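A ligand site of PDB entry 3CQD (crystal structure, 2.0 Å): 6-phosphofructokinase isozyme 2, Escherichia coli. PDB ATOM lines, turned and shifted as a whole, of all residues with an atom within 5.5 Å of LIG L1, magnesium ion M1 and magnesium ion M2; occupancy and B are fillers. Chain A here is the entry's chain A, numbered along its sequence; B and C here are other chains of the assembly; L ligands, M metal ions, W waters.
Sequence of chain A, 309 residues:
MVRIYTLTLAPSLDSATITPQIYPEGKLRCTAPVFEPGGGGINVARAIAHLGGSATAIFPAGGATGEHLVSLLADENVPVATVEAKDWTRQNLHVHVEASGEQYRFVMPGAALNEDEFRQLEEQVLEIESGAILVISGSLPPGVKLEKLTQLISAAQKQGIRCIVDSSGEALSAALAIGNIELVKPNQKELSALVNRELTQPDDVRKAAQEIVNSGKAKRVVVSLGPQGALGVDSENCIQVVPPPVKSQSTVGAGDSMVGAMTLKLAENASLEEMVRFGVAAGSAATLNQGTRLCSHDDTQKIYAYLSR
An oxygen (O12) of LIG L1 sits at hydrogen-bond distance from the backbone carbonyl oxygen (O) of Gly 229 (2.5 Å).
N of Gly 226 sits at hydrogen-bond distance from O8 of LIG L1 (2.8 Å).
The side-chain amino group of Lys 185 lies close to an oxygen (O5) of LIG L1.
The side-chain hydroxyl (OG) of Ser 224 lies within hydrogen-bond range of an oxygen (O8) of LIG L1, 2.8 Å away.
NZ of Lys 27 of chain B lies close to O1 of LIG L1 (2.8 Å).
O13 of LIG L1 is in hydrogen-bond range of OG of Ser 284.
The side-chain amide nitrogen (ND2) of Asn 187 sits close to an oxygen (O4) of LIG L1 (2.9 Å).
The backbone NH (N) of Gly 255 lies within hydrogen-bond range of an oxygen (O2) of LIG L1 (2.9 Å).
The side-chain hydroxyl (OG) of Ser 248 lies within hydrogen-bond range of a nitrogen (N3) of LIG L1.
SD of Met 258 sits close to O12 of LIG L1.
An oxygen (O13) of LIG L1 sits at hydrogen-bond distance from the backbone carbonyl oxygen of Val 280 (3.0 Å).
The backbone NH (N) of Leu 225 is in hydrogen-bond range of an oxygen (O8) of LIG L1 (3.2 Å).
O2 of LIG L1 lies within hydrogen-bond range of N of Ala 254 (3.4 Å).
The backbone NH (N) of Lys 27 of chain B is in hydrogen-bond range of an oxygen (O5) of LG2 L2, 2.7 Å away.
The side-chain amino group (NZ) of Lys 27 of chain B lies within salt-bridge range of an oxygen (O1) of LG2 L2, 2.9 Å away.
The side-chain amide nitrogen (ND2) of Asn 187 sits at hydrogen-bond distance from an oxygen (O2) of LG2 L2 (3.0 Å).
OG of Ser 224 lies within hydrogen-bond range of NZ of Lys 185 (2.7 Å).
The side-chain hydroxyl of Ser 284 lies within hydrogen-bond range of the backbone carbonyl oxygen of Val 280 (3.0 Å).
OG1 of Thr 287 lies within hydrogen-bond range of O of Ser 284 (2.6 Å).
OD1 of Asn 187 sits at hydrogen-bond distance from N of Glu 190 (2.8 Å).
The backbone carbonyl oxygen (O) of Thr 287 sits at hydrogen-bond distance from the backbone NH (N) of Ser 250, 3.0 Å away.
The backbone carbonyl oxygen of Pro 227 lies within hydrogen-bond range of the side-chain amide nitrogen of Gln 228 of chain C (2.8 Å).
O of Gly 283 sits close to O11 of LIG L1.
Pro 227 touches LIG L1.
CG of Pro 243 touches N5 of LIG L1, 3.96 Å away.
O of Thr 251 touches O2 of LIG L1, at 3.9 Å.
Gly 253 touches LIG L1 (N to O2, 3.99 Å).
Thr 287 touches LIG L1.
Within 4 Å of LIG L1: Lys 185, Asn 187, Ser 224, Leu 225, Gly 226, Pro 227, Gly 229, Pro 243, Ser 248, Thr 251, Gly 253, Ala 254, Gly 255, Met 258, Val 280, Gly 283, Ser 284, Thr 287 and Lys 27 of chain B.
The nearest printed residue that does not touch LIG L1 is Ala 230 (4.1 Å).
Asp 166 touches magnesium ion M1 (OD1 to MG, 3.9 Å).
Lys 185 touches magnesium ion M1 (NZ to MG, 3.95 Å).
Lys 27 of chain B touches magnesium ion M1.
Of the 30 residues printed, 3 come within 4 Å of magnesium ion M1.
Along chain A the residues within 4 Å of magnesium ion M1 span positions 166 to 185.
The nearest printed residue that does not touch magnesium ion M1 is Glu 190 (4.02 Å).
Residues that only touch magnesium ion M2: Asn 187 (3.7 Å).
The nearest printed residue that does not touch magnesium ion M2 is Lys 27 of chain B (4.3 Å).
Magnesium ion M1 is bound by O5 of LIG L1 (2.0 Å), water W3 (2.0 Å), water W9 (2.1 Å), O1 of LIG L1 (2.1 Å), water W12 (2.1 Å) and water W13 (2.1 Å).
Magnesium ion M2 is bound by an oxygen (O3) of LG2 L2 (2.0 Å).
Magnesium ion M2 is bound by water W5 (2.0 Å).
O3 of LIG L1 binds magnesium ion M2 (2.1 Å).
Magnesium ion M2 is bound by an oxygen (O4) of LG2 L2 (2.1 Å).
Magnesium ion M2 is bound by O4 of LIG L1 (2.1 Å).
Magnesium ion M2 is bound by water W7 (2.1 Å).
Magnesium ion M2 has six donor atoms within binding distance.
Water W9 lies within hydrogen-bond range of OE2 of Glu 190 (2.7 Å), ND2 of Asn 187 (3.1 Å), NZ of Lys 27 of chain B (3.4 Å) and O1 of LG2 L2 (3.4 Å).
Water W5 lies within hydrogen-bond range of an oxygen (O7) of LIG L1 (2.6 Å) and a nitrogen (N3) of LG2 L2 (3.2 Å).
Water W2 lies within hydrogen-bond range of O2 of LIG L1, N of Asp 256 and N of Gly 255.
Water W4 lies within hydrogen-bond range of the guanidinium group of Arg 105, the side-chain hydroxyl of Thr 251 and an oxygen (O2) of LIG L1.
Water W8 lies within hydrogen-bond range of the guanidinium group (NH2) of Arg 105 (2.6 Å), an oxygen (O2) of LIG L1 (2.7 Å) and the backbone NH (N) of Gly 253 (2.8 Å).
Water W10 lies within hydrogen-bond range of N3 of LIG L1 (3.1 Å) and OG of Ser 248 (3.4 Å).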
ATOM      1  N   ARG A 105      -8.393 -13.793  -1.562  1.00  0.00           N
ATOM      2  CA  ARG A 105      -7.698 -13.801  -2.822  1.00  0.00           C
ATOM      3  C   ARG A 105      -8.172 -12.635  -3.611  1.00  0.00           C
ATOM      4  O   ARG A 105      -9.326 -12.621  -4.068  1.00  0.00           O
ATOM      5  CB  ARG A 105      -7.995 -15.086  -3.586  1.00  0.00           C
ATOM      6  CG  ARG A 105      -7.616 -16.311  -2.826  1.00  0.00           C
ATOM      7  CD  ARG A 105      -8.552 -17.416  -3.211  1.00  0.00           C
ATOM      8  NE  ARG A 105      -8.128 -18.022  -4.451  1.00  0.00           N
ATOM      9  CZ  ARG A 105      -8.831 -18.898  -5.160  1.00  0.00           C
ATOM     10  NH1 ARG A 105     -10.040 -19.297  -4.779  1.00  0.00           N
ATOM     11  NH2 ARG A 105      -8.290 -19.384  -6.258  1.00  0.00           N
ATOM     12  N   ASP A 166      -9.597 -23.229 -20.794  1.00  0.00           N
ATOM     13  CA  ASP A 166     -10.199 -22.971 -19.508  1.00  0.00           C
ATOM     14  C   ASP A 166     -10.197 -21.472 -19.297  1.00  0.00           C
ATOM     15  O   ASP A 166      -9.167 -20.859 -19.028  1.00  0.00           O
ATOM     16  CB  ASP A 166      -9.460 -23.690 -18.386  1.00  0.00           C
ATOM     17  CG  ASP A 166     -10.035 -23.396 -17.011  1.00  0.00           C
ATOM     18  OD1 ASP A 166      -9.539 -23.949 -16.025  1.00  0.00           O
ATOM     19  OD2 ASP A 166     -10.981 -22.599 -16.902  1.00  0.00           O
ATOM     20  N   LYS A 185     -13.094 -26.880 -19.976  1.00  0.00           N
ATOM     21  CA  LYS A 185     -13.520 -27.141 -18.596  1.00  0.00           C
ATOM     22  C   LYS A 185     -14.155 -25.892 -17.997  1.00  0.00           C
ATOM     23  O   LYS A 185     -13.498 -25.172 -17.247  1.00  0.00           O
ATOM     24  CB  LYS A 185     -12.354 -27.631 -17.703  1.00  0.00           C
ATOM     25  CG  LYS A 185     -12.853 -28.106 -16.282  1.00  0.00           C
ATOM     26  CD  LYS A 185     -11.802 -27.879 -15.195  1.00  0.00           C
ATOM     27  CE  LYS A 185     -11.733 -26.406 -14.701  1.00  0.00           C
ATOM     28  NZ  LYS A 185     -13.054 -25.701 -14.453  1.00  0.00           N
ATOM     29  N   ASN A 187     -16.395 -24.206 -15.182  1.00  0.00           N
ATOM     30  CA  ASN A 187     -17.117 -24.542 -13.964  1.00  0.00           C
ATOM     31  C   ASN A 187     -18.577 -24.178 -14.211  1.00  0.00           C
ATOM     32  O   ASN A 187     -18.945 -23.840 -15.337  1.00  0.00           O
ATOM     33  CB  ASN A 187     -16.520 -23.896 -12.713  1.00  0.00           C
ATOM     34  CG  ASN A 187     -16.622 -22.393 -12.721  1.00  0.00           C
ATOM     35  OD1 ASN A 187     -17.379 -21.797 -13.490  1.00  0.00           O
ATOM     36  ND2 ASN A 187     -15.846 -21.763 -11.868  1.00  0.00           N
ATOM     37  N   GLU A 190     -19.182 -20.556 -15.259  1.00  0.00           N
ATOM     38  CA  GLU A 190     -18.598 -20.358 -16.582  1.00  0.00           C
ATOM     39  C   GLU A 190     -19.456 -21.006 -17.676  1.00  0.00           C
ATOM     40  O   GLU A 190     -19.634 -20.442 -18.743  1.00  0.00           O
ATOM     41  CB  GLU A 190     -17.142 -20.867 -16.638  1.00  0.00           C
ATOM     42  CG  GLU A 190     -16.224 -20.063 -15.719  1.00  0.00           C
ATOM     43  CD  GLU A 190     -14.896 -20.730 -15.376  1.00  0.00           C
ATOM     44  OE1 GLU A 190     -14.696 -21.944 -15.576  1.00  0.00           O
ATOM     45  OE2 GLU A 190     -14.028 -20.004 -14.840  1.00  0.00           O
ATOM     46  N   SER A 224     -16.844 -28.709 -14.383  1.00  0.00           N
ATOM     47  CA  SER A 224     -16.400 -28.978 -13.024  1.00  0.00           C
ATOM     48  C   SER A 224     -17.400 -28.370 -12.048  1.00  0.00           C
ATOM     49  O   SER A 224     -17.960 -27.291 -12.276  1.00  0.00           O
ATOM     50  CB  SER A 224     -14.953 -28.524 -12.800  1.00  0.00           C
ATOM     51  OG  SER A 224     -14.801 -27.126 -12.913  1.00  0.00           O
ATOM     52  N   LEU A 225     -17.645 -29.107 -10.971  1.00  0.00           N
ATOM     53  CA  LEU A 225     -18.803 -28.852 -10.136  1.00  0.00           C
ATOM     54  C   LEU A 225     -18.368 -28.688  -8.702  1.00  0.00           C
ATOM     55  O   LEU A 225     -19.137 -28.985  -7.790  1.00  0.00           O
ATOM     56  CB  LEU A 225     -19.774 -30.042 -10.260  1.00  0.00           C
ATOM     57  CG  LEU A 225     -20.242 -30.394 -11.669  1.00  0.00           C
ATOM     58  CD1 LEU A 225     -21.064 -31.695 -11.687  1.00  0.00           C
ATOM     59  CD2 LEU A 225     -21.035 -29.247 -12.230  1.00  0.00           C
ATOM     60  N   GLY A 226     -17.132 -28.238  -8.516  1.00  0.00           N
ATOM     61  CA  GLY A 226     -16.571 -28.007  -7.197  1.00  0.00           C
ATOM     62  C   GLY A 226     -16.580 -29.297  -6.389  1.00  0.00           C
ATOM     63  O   GLY A 226     -16.113 -30.316  -6.847  1.00  0.00           O
ATOM     64  N   PRO A 227     -17.194 -29.271  -5.189  1.00  0.00           N
ATOM     65  CA  PRO A 227     -17.202 -30.493  -4.381  1.00  0.00           C
ATOM     66  C   PRO A 227     -17.966 -31.637  -5.066  1.00  0.00           C
ATOM     67  O   PRO A 227     -17.843 -32.799  -4.666  1.00  0.00           O
ATOM     68  CB  PRO A 227     -17.927 -30.069  -3.099  1.00  0.00           C
ATOM     69  CG  PRO A 227     -18.801 -28.899  -3.555  1.00  0.00           C
ATOM     70  CD  PRO A 227     -17.954 -28.173  -4.549  1.00  0.00           C
ATOM     71  N   GLY A 229     -17.573 -32.625  -8.098  1.00  0.00           N
ATOM     72  CA  GLY A 229     -16.694 -33.304  -9.043  1.00  0.00           C
ATOM     73  C   GLY A 229     -16.808 -32.634 -10.398  1.00  0.00           C
ATOM     74  O   GLY A 229     -16.610 -31.432 -10.534  1.00  0.00           O
ATOM     75  N   ALA A 230     -17.178 -33.427 -11.397  1.00  0.00           N
ATOM     76  CA  ALA A 230     -17.222 -32.927 -12.748  1.00  0.00           C
ATOM     77  C   ALA A 230     -18.123 -33.833 -13.557  1.00  0.00           C
ATOM     78  O   ALA A 230     -18.244 -35.030 -13.262  1.00  0.00           O
ATOM     79  CB  ALA A 230     -15.802 -32.892 -13.369  1.00  0.00           C
ATOM     80  N   PRO A 243     -15.819 -36.612  -6.238  1.00  0.00           N
ATOM     81  CA  PRO A 243     -14.676 -36.928  -5.403  1.00  0.00           C
ATOM     82  C   PRO A 243     -15.148 -37.627  -4.158  1.00  0.00           C
ATOM     83  O   PRO A 243     -16.332 -37.513  -3.799  1.00  0.00           O
ATOM     84  CB  PRO A 243     -14.095 -35.548  -5.041  1.00  0.00           C
ATOM     85  CG  PRO A 243     -15.166 -34.586  -5.296  1.00  0.00           C
ATOM     86  CD  PRO A 243     -16.080 -35.158  -6.302  1.00  0.00           C
ATOM     87  N   VAL A 246     -14.451 -36.340   1.374  1.00  0.00           N
ATOM     88  CA  VAL A 246     -13.300 -35.860   2.107  1.00  0.00           C
ATOM     89  C   VAL A 246     -13.237 -34.331   2.117  1.00  0.00           C
ATOM     90  O   VAL A 246     -13.656 -33.684   1.140  1.00  0.00           O
ATOM     91  CB  VAL A 246     -12.002 -36.428   1.505  1.00  0.00           C
ATOM     92  CG1 VAL A 246     -10.771 -35.801   2.160  1.00  0.00           C
ATOM     93  CG2 VAL A 246     -11.973 -37.953   1.641  1.00  0.00           C
ATOM     94  N   SER A 248     -13.326 -30.497   2.116  1.00  0.00           N
ATOM     95  CA  SER A 248     -12.036 -29.969   1.645  1.00  0.00           C
ATOM     96  C   SER A 248     -11.564 -28.828   2.545  1.00  0.00           C
ATOM     97  O   SER A 248     -12.335 -28.315   3.356  1.00  0.00           O
ATOM     98  CB  SER A 248     -12.215 -29.446   0.233  1.00  0.00           C
ATOM     99  OG  SER A 248     -13.261 -28.479   0.215  1.00  0.00           O
ATOM    100  N   SER A 250      -9.255 -26.144   1.196  1.00  0.00           N
ATOM    101  CA  SER A 250      -9.016 -24.967   0.360  1.00  0.00           C
ATOM    102  C   SER A 250      -9.558 -25.274  -1.012  1.00  0.00           C
ATOM    103  O   SER A 250      -9.787 -26.428  -1.344  1.00  0.00           O
ATOM    104  CB  SER A 250      -7.517 -24.662   0.302  1.00  0.00           C
ATOM    105  OG  SER A 250      -7.260 -23.544  -0.514  1.00  0.00           O
ATOM    106  N   THR A 251      -9.799 -24.256  -1.825  1.00  0.00           N
ATOM    107  CA  THR A 251     -10.220 -24.514  -3.199  1.00  0.00           C
ATOM    108  C   THR A 251      -9.150 -24.036  -4.183  1.00  0.00           C
ATOM    109  O   THR A 251      -9.256 -24.290  -5.371  1.00  0.00           O
ATOM    110  CB  THR A 251     -11.593 -23.869  -3.531  1.00  0.00           C
ATOM    111  OG1 THR A 251     -11.475 -22.443  -3.504  1.00  0.00           O
ATOM    112  CG2 THR A 251     -12.656 -24.307  -2.540  1.00  0.00           C
ATOM    113  N   VAL A 252      -8.136 -23.341  -3.664  1.00  0.00           N
ATOM    114  CA  VAL A 252      -7.111 -22.751  -4.518  1.00  0.00           C
ATOM    115  C   VAL A 252      -6.393 -23.795  -5.354  1.00  0.00           C
ATOM    116  O   VAL A 252      -5.902 -24.820  -4.846  1.00  0.00           O
ATOM    117  CB  VAL A 252      -6.111 -21.858  -3.733  1.00  0.00           C
ATOM    118  CG1 VAL A 252      -5.158 -21.107  -4.714  1.00  0.00           C
ATOM    119  CG2 VAL A 252      -6.856 -20.850  -2.896  1.00  0.00           C
ATOM    120  N   GLY A 253      -6.386 -23.541  -6.662  1.00  0.00           N
ATOM    121  CA  GLY A 253      -5.658 -24.357  -7.579  1.00  0.00           C
ATOM    122  C   GLY A 253      -6.444 -25.567  -8.034  1.00  0.00           C
ATOM    123  O   GLY A 253      -5.901 -26.404  -8.723  1.00  0.00           O
ATOM    124  N   ALA A 254      -7.715 -25.666  -7.620  1.00  0.00           N
ATOM    125  CA  ALA A 254      -8.553 -26.835  -7.895  1.00  0.00           C
ATOM    126  C   ALA A 254      -8.745 -26.987  -9.404  1.00  0.00           C
ATOM    127  O   ALA A 254      -8.520 -28.059  -9.951  1.00  0.00           O
ATOM    128  CB  ALA A 254      -9.910 -26.727  -7.205  1.00  0.00           C
ATOM    129  N   GLY A 255      -9.181 -25.909 -10.045  1.00  0.00           N
ATOM    130  CA  GLY A 255      -9.446 -25.949 -11.487  1.00  0.00           C
ATOM    131  C   GLY A 255      -8.216 -26.276 -12.316  1.00  0.00           C
ATOM    132  O   GLY A 255      -8.267 -27.120 -13.199  1.00  0.00           O
ATOM    133  N   ASP A 256      -7.103 -25.597 -12.031  1.00  0.00           N
ATOM    134  CA  ASP A 256      -5.880 -25.767 -12.823  1.00  0.00           C
ATOM    135  C   ASP A 256      -5.291 -27.160 -12.650  1.00  0.00           C
ATOM    136  O   ASP A 256      -4.748 -27.726 -13.594  1.00  0.00           O
ATOM    137  CB  ASP A 256      -4.858 -24.693 -12.492  1.00  0.00           C
ATOM    138  CG  ASP A 256      -5.345 -23.288 -12.821  1.00  0.00           C
ATOM    139  OD1 ASP A 256      -4.997 -22.334 -12.117  1.00  0.00           O
ATOM    140  OD2 ASP A 256      -6.114 -23.144 -13.778  1.00  0.00           O
ATOM    141  N   MET A 258      -7.062 -29.858 -11.885  1.00  0.00           N
ATOM    142  CA  MET A 258      -7.926 -30.702 -12.684  1.00  0.00           C
ATOM    143  C   MET A 258      -7.576 -30.620 -14.176  1.00  0.00           C
ATOM    144  O   MET A 258      -7.423 -31.639 -14.833  1.00  0.00           O
ATOM    145  CB  MET A 258      -9.395 -30.323 -12.478  1.00  0.00           C
ATOM    146  CG  MET A 258     -10.293 -30.935 -13.541  1.00  0.00           C
ATOM    147  SD  MET A 258     -12.022 -30.665 -13.220  1.00  0.00           S
ATOM    148  CE  MET A 258     -12.389 -32.109 -12.239  1.00  0.00           C
ATOM    149  N   GLY A 279      -8.895 -35.951 -13.512  1.00  0.00           N
ATOM    150  CA  GLY A 279      -9.167 -34.531 -13.290  1.00  0.00           C
ATOM    151  C   GLY A 279      -9.755 -34.277 -11.914  1.00  0.00           C
ATOM    152  O   GLY A 279      -9.332 -33.368 -11.187  1.00  0.00           O
ATOM    153  N   VAL A 280     -10.743 -35.080 -11.553  1.00  0.00           N
ATOM    154  CA  VAL A 280     -11.396 -34.906 -10.264  1.00  0.00           C
ATOM    155  C   VAL A 280     -10.414 -35.238  -9.144  1.00  0.00           C
ATOM    156  O   VAL A 280     -10.396 -34.559  -8.117  1.00  0.00           O
ATOM    157  CB  VAL A 280     -12.698 -35.731 -10.131  1.00  0.00           C
ATOM    158  CG1 VAL A 280     -13.128 -35.848  -8.651  1.00  0.00           C
ATOM    159  CG2 VAL A 280     -13.808 -35.097 -10.947  1.00  0.00           C
ATOM    160  N   ALA A 281      -9.609 -36.276  -9.347  1.00  0.00           N
ATOM    161  CA  ALA A 281      -8.599 -36.653  -8.374  1.00  0.00           C
ATOM    162  C   ALA A 281      -7.621 -35.512  -8.124  1.00  0.00           C
ATOM    163  O   ALA A 281      -7.309 -35.201  -6.976  1.00  0.00           O
ATOM    164  CB  ALA A 281      -7.865 -37.897  -8.803  1.00  0.00           C
ATOM    165  N   GLY A 283      -7.981 -32.226  -8.971  1.00  0.00           N
ATOM    166  CA  GLY A 283      -8.675 -31.040  -8.482  1.00  0.00           C
ATOM    167  C   GLY A 283      -8.924 -31.199  -6.997  1.00  0.00           C
ATOM    168  O   GLY A 283      -8.699 -30.280  -6.205  1.00  0.00           O
ATOM    169  N   SER A 284      -9.386 -32.389  -6.617  1.00  0.00           N
ATOM    170  CA  SER A 284      -9.720 -32.641  -5.224  1.00  0.00           C
ATOM    171  C   SER A 284      -8.478 -32.752  -4.340  1.00  0.00           C
ATOM    172  O   SER A 284      -8.505 -32.273  -3.211  1.00  0.00           O
ATOM    173  CB  SER A 284     -10.653 -33.830  -5.111  1.00  0.00           C
ATOM    174  OG  SER A 284     -11.905 -33.486  -5.710  1.00  0.00           O
ATOM    175  N   THR A 287      -7.425 -29.551  -3.190  1.00  0.00           N
ATOM    176  CA  THR A 287      -8.241 -28.952  -2.145  1.00  0.00           C
ATOM    177  C   THR A 287      -7.828 -29.356  -0.729  1.00  0.00           C
ATOM    178  O   THR A 287      -8.459 -28.915   0.239  1.00  0.00           O
ATOM    179  CB  THR A 287      -9.758 -29.218  -2.330  1.00  0.00           C
ATOM    180  OG1 THR A 287     -10.041 -30.584  -2.003  1.00  0.00           O
ATOM    181  CG2 THR A 287     -10.190 -28.890  -3.736  1.00  0.00           C
ATOM    182  N   LYS B  27     -12.198 -16.319  -5.286  1.00  0.00           N
ATOM    183  CA  LYS B  27     -11.473 -15.297  -6.001  1.00  0.00           C
ATOM    184  C   LYS B  27     -12.301 -14.040  -5.974  1.00  0.00           C
ATOM    185  O   LYS B  27     -13.420 -14.009  -6.482  1.00  0.00           O
ATOM    186  CB  LYS B  27     -11.274 -15.706  -7.447  1.00  0.00           C
ATOM    187  CG  LYS B  27     -10.476 -16.940  -7.656  1.00  0.00           C
ATOM    188  CD  LYS B  27     -10.663 -17.410  -9.097  1.00  0.00           C
ATOM    189  CE  LYS B  27     -10.543 -18.905  -9.218  1.00  0.00           C
ATOM    190  NZ  LYS B  27     -10.888 -19.333 -10.595  1.00  0.00           N
ATOM    191  N   GLN C 228     -22.173 -32.854  -1.567  1.00  0.00           N
ATOM    192  CA  GLN C 228     -21.777 -34.146  -2.101  1.00  0.00           C
ATOM    193  C   GLN C 228     -22.870 -35.169  -1.928  1.00  0.00           C
ATOM    194  O   GLN C 228     -22.694 -36.320  -2.304  1.00  0.00           O
ATOM    195  CB  GLN C 228     -20.465 -34.620  -1.479  1.00  0.00           C
ATOM    196  CG  GLN C 228     -19.311 -33.724  -1.881  1.00  0.00           C
ATOM    197  CD  GLN C 228     -17.951 -34.253  -1.459  1.00  0.00           C
ATOM    198  OE1 GLN C 228     -17.814 -35.028  -0.511  1.00  0.00           O
ATOM    199  NE2 GLN C 228     -16.923 -33.814  -2.176  1.00  0.00           N
HETATM  200  P1  LIG L   1     -10.789 -22.662  -9.753  1.00  0.00           P
HETATM  201  O1  LIG L   1     -10.544 -22.078 -11.113  1.00  0.00           O
HETATM  202  O2  LIG L   1      -9.496 -23.150  -9.138  1.00  0.00           O
HETATM  203  O3  LIG L   1     -11.682 -21.805  -8.915  1.00  0.00           O
HETATM  204  P2  LIG L   1     -12.955 -24.216 -10.883  1.00  0.00           P
HETATM  205  O4  LIG L   1     -14.060 -23.363 -10.324  1.00  0.00           O
HETATM  206  O5  LIG L   1     -12.544 -23.978 -12.309  1.00  0.00           O
HETATM  207  O6  LIG L   1     -11.612 -24.032  -9.980  1.00  0.00           O
HETATM  208  P3  LIG L   1     -13.958 -26.571  -9.479  1.00  0.00           P
HETATM  209  O7  LIG L   1     -14.244 -25.667  -8.327  1.00  0.00           O
HETATM  210  O8  LIG L   1     -15.052 -27.369 -10.130  1.00  0.00           O
HETATM  211  O9  LIG L   1     -13.296 -25.775 -10.739  1.00  0.00           O
HETATM  212  O10 LIG L   1     -12.681 -27.458  -9.132  1.00  0.00           O
HETATM  213  C1  LIG L   1     -12.142 -28.434 -10.048  1.00  0.00           C
HETATM  214  C2  LIG L   1     -12.143 -29.787  -9.379  1.00  0.00           C
HETATM  215  O11 LIG L   1     -11.548 -29.611  -8.096  1.00  0.00           O
HETATM  216  C3  LIG L   1     -13.513 -30.374  -9.040  1.00  0.00           C
HETATM  217  O12 LIG L   1     -14.158 -31.009 -10.151  1.00  0.00           O
HETATM  218  C4  LIG L   1     -13.184 -31.310  -7.891  1.00  0.00           C
HETATM  219  O13 LIG L   1     -12.535 -32.518  -8.310  1.00  0.00           O
HETATM  220  C5  LIG L   1     -12.133 -30.508  -7.153  1.00  0.00           C
HETATM  221  N1  LIG L   1     -12.776 -29.686  -6.113  1.00  0.00           N
HETATM  222  C6  LIG L   1     -13.078 -28.397  -6.206  1.00  0.00           C
HETATM  223  N2  LIG L   1     -13.682 -27.943  -5.088  1.00  0.00           N
HETATM  224  C7  LIG L   1     -13.778 -28.985  -4.260  1.00  0.00           C
HETATM  225  C8  LIG L   1     -14.297 -29.188  -2.894  1.00  0.00           C
HETATM  226  N3  LIG L   1     -14.828 -28.141  -2.238  1.00  0.00           N
HETATM  227  N4  LIG L   1     -14.203 -30.434  -2.360  1.00  0.00           N
HETATM  228  C9  LIG L   1     -13.649 -31.459  -3.035  1.00  0.00           C
HETATM  229  N5  LIG L   1     -13.148 -31.332  -4.271  1.00  0.00           N
HETATM  230  C10 LIG L   1     -13.181 -30.145  -4.916  1.00  0.00           C
HETATM  231  P1  LG2 L   2     -14.403 -19.046 -10.282  1.00  0.00           P
HETATM  232  O1  LG2 L   2     -13.498 -18.109 -11.020  1.00  0.00           O
HETATM  233  O2  LG2 L   2     -15.842 -18.968 -10.681  1.00  0.00           O
HETATM  234  O3  LG2 L   2     -13.900 -20.470 -10.219  1.00  0.00           O
HETATM  235  P2  LG2 L   2     -14.377 -19.111  -7.388  1.00  0.00           P
HETATM  236  O4  LG2 L   2     -13.650 -20.425  -7.347  1.00  0.00           O
HETATM  237  O5  LG2 L   2     -13.959 -18.045  -6.444  1.00  0.00           O
HETATM  238  O6  LG2 L   2     -14.310 -18.392  -8.828  1.00  0.00           O
HETATM  239  P3  LG2 L   2     -17.115 -18.495  -6.800  1.00  0.00           P
HETATM  240  O7  LG2 L   2     -16.860 -17.076  -7.277  1.00  0.00           O
HETATM  241  O8  LG2 L   2     -18.457 -19.080  -7.161  1.00  0.00           O
HETATM  242  O9  LG2 L   2     -15.939 -19.469  -7.279  1.00  0.00           O
HETATM  243  O10 LG2 L   2     -16.930 -18.584  -5.207  1.00  0.00           O
HETATM  244  C1  LG2 L   2     -17.695 -17.723  -4.377  1.00  0.00           C
HETATM  245  C2  LG2 L   2     -18.040 -18.467  -3.095  1.00  0.00           C
HETATM  246  O11 LG2 L   2     -18.531 -19.781  -3.388  1.00  0.00           O
HETATM  247  C3  LG2 L   2     -16.817 -18.613  -2.218  1.00  0.00           C
HETATM  248  O12 LG2 L   2     -17.060 -17.825  -1.063  1.00  0.00           O
HETATM  249  C4  LG2 L   2     -16.708 -20.080  -1.889  1.00  0.00           C
HETATM  250  O13 LG2 L   2     -16.929 -20.306  -0.491  1.00  0.00           O
HETATM  251  C5  LG2 L   2     -17.778 -20.784  -2.695  1.00  0.00           C
HETATM  252  N1  LG2 L   2     -17.126 -21.734  -3.634  1.00  0.00           N
HETATM  253  C6  LG2 L   2     -16.783 -21.522  -4.927  1.00  0.00           C
HETATM  254  N2  LG2 L   2     -16.176 -22.609  -5.483  1.00  0.00           N
HETATM  255  C7  LG2 L   2     -16.125 -23.550  -4.523  1.00  0.00           C
HETATM  256  C8  LG2 L   2     -15.617 -24.938  -4.410  1.00  0.00           C
HETATM  257  N3  LG2 L   2     -15.038 -25.531  -5.464  1.00  0.00           N
HETATM  258  N4  LG2 L   2     -15.749 -25.581  -3.237  1.00  0.00           N
HETATM  259  C9  LG2 L   2     -16.332 -25.002  -2.173  1.00  0.00           C
HETATM  260  N5  LG2 L   2     -16.807 -23.738  -2.188  1.00  0.00           N
HETATM  261  C10 LG2 L   2     -16.740 -22.978  -3.315  1.00  0.00           C
HETATM  262 MG    MG M   1     -11.443 -22.421 -12.941  1.00  0.00          MG
HETATM  263 MG    MG M   2     -13.756 -21.932  -8.807  1.00  0.00          MG
HETATM  264  O   HOH W   1     -16.762 -24.438  -8.546  1.00  0.00           O
HETATM  265  O   HOH W   2      -7.246 -23.394 -10.375  1.00  0.00           O
HETATM  266  O   HOH W   3      -9.894 -23.594 -13.527  1.00  0.00           O
HETATM  267  O   HOH W   4     -10.977 -21.624  -6.376  1.00  0.00           O
HETATM  268  O   HOH W   5     -13.544 -23.372  -7.366  1.00  0.00           O
HETATM  269  O   HOH W   6     -14.157 -34.425  -1.585  1.00  0.00           O
HETATM  270  O   HOH W   7     -15.877 -22.068  -8.633  1.00  0.00           O
HETATM  271  O   HOH W   8      -7.876 -21.427  -7.809  1.00  0.00           O
HETATM  272  O   HOH W   9     -12.955 -21.070 -12.598  1.00  0.00           O
HETATM  273  O   HOH W  10     -16.633 -28.139   0.314  1.00  0.00           O
HETATM  274  O   HOH W  11     -15.231 -31.314   0.016  1.00  0.00           O
HETATM  275  O   HOH W  12     -10.323 -20.869 -13.849  1.00  0.00           O
HETATM  276  O   HOH W  13     -12.447 -22.740 -14.794  1.00  0.00           O
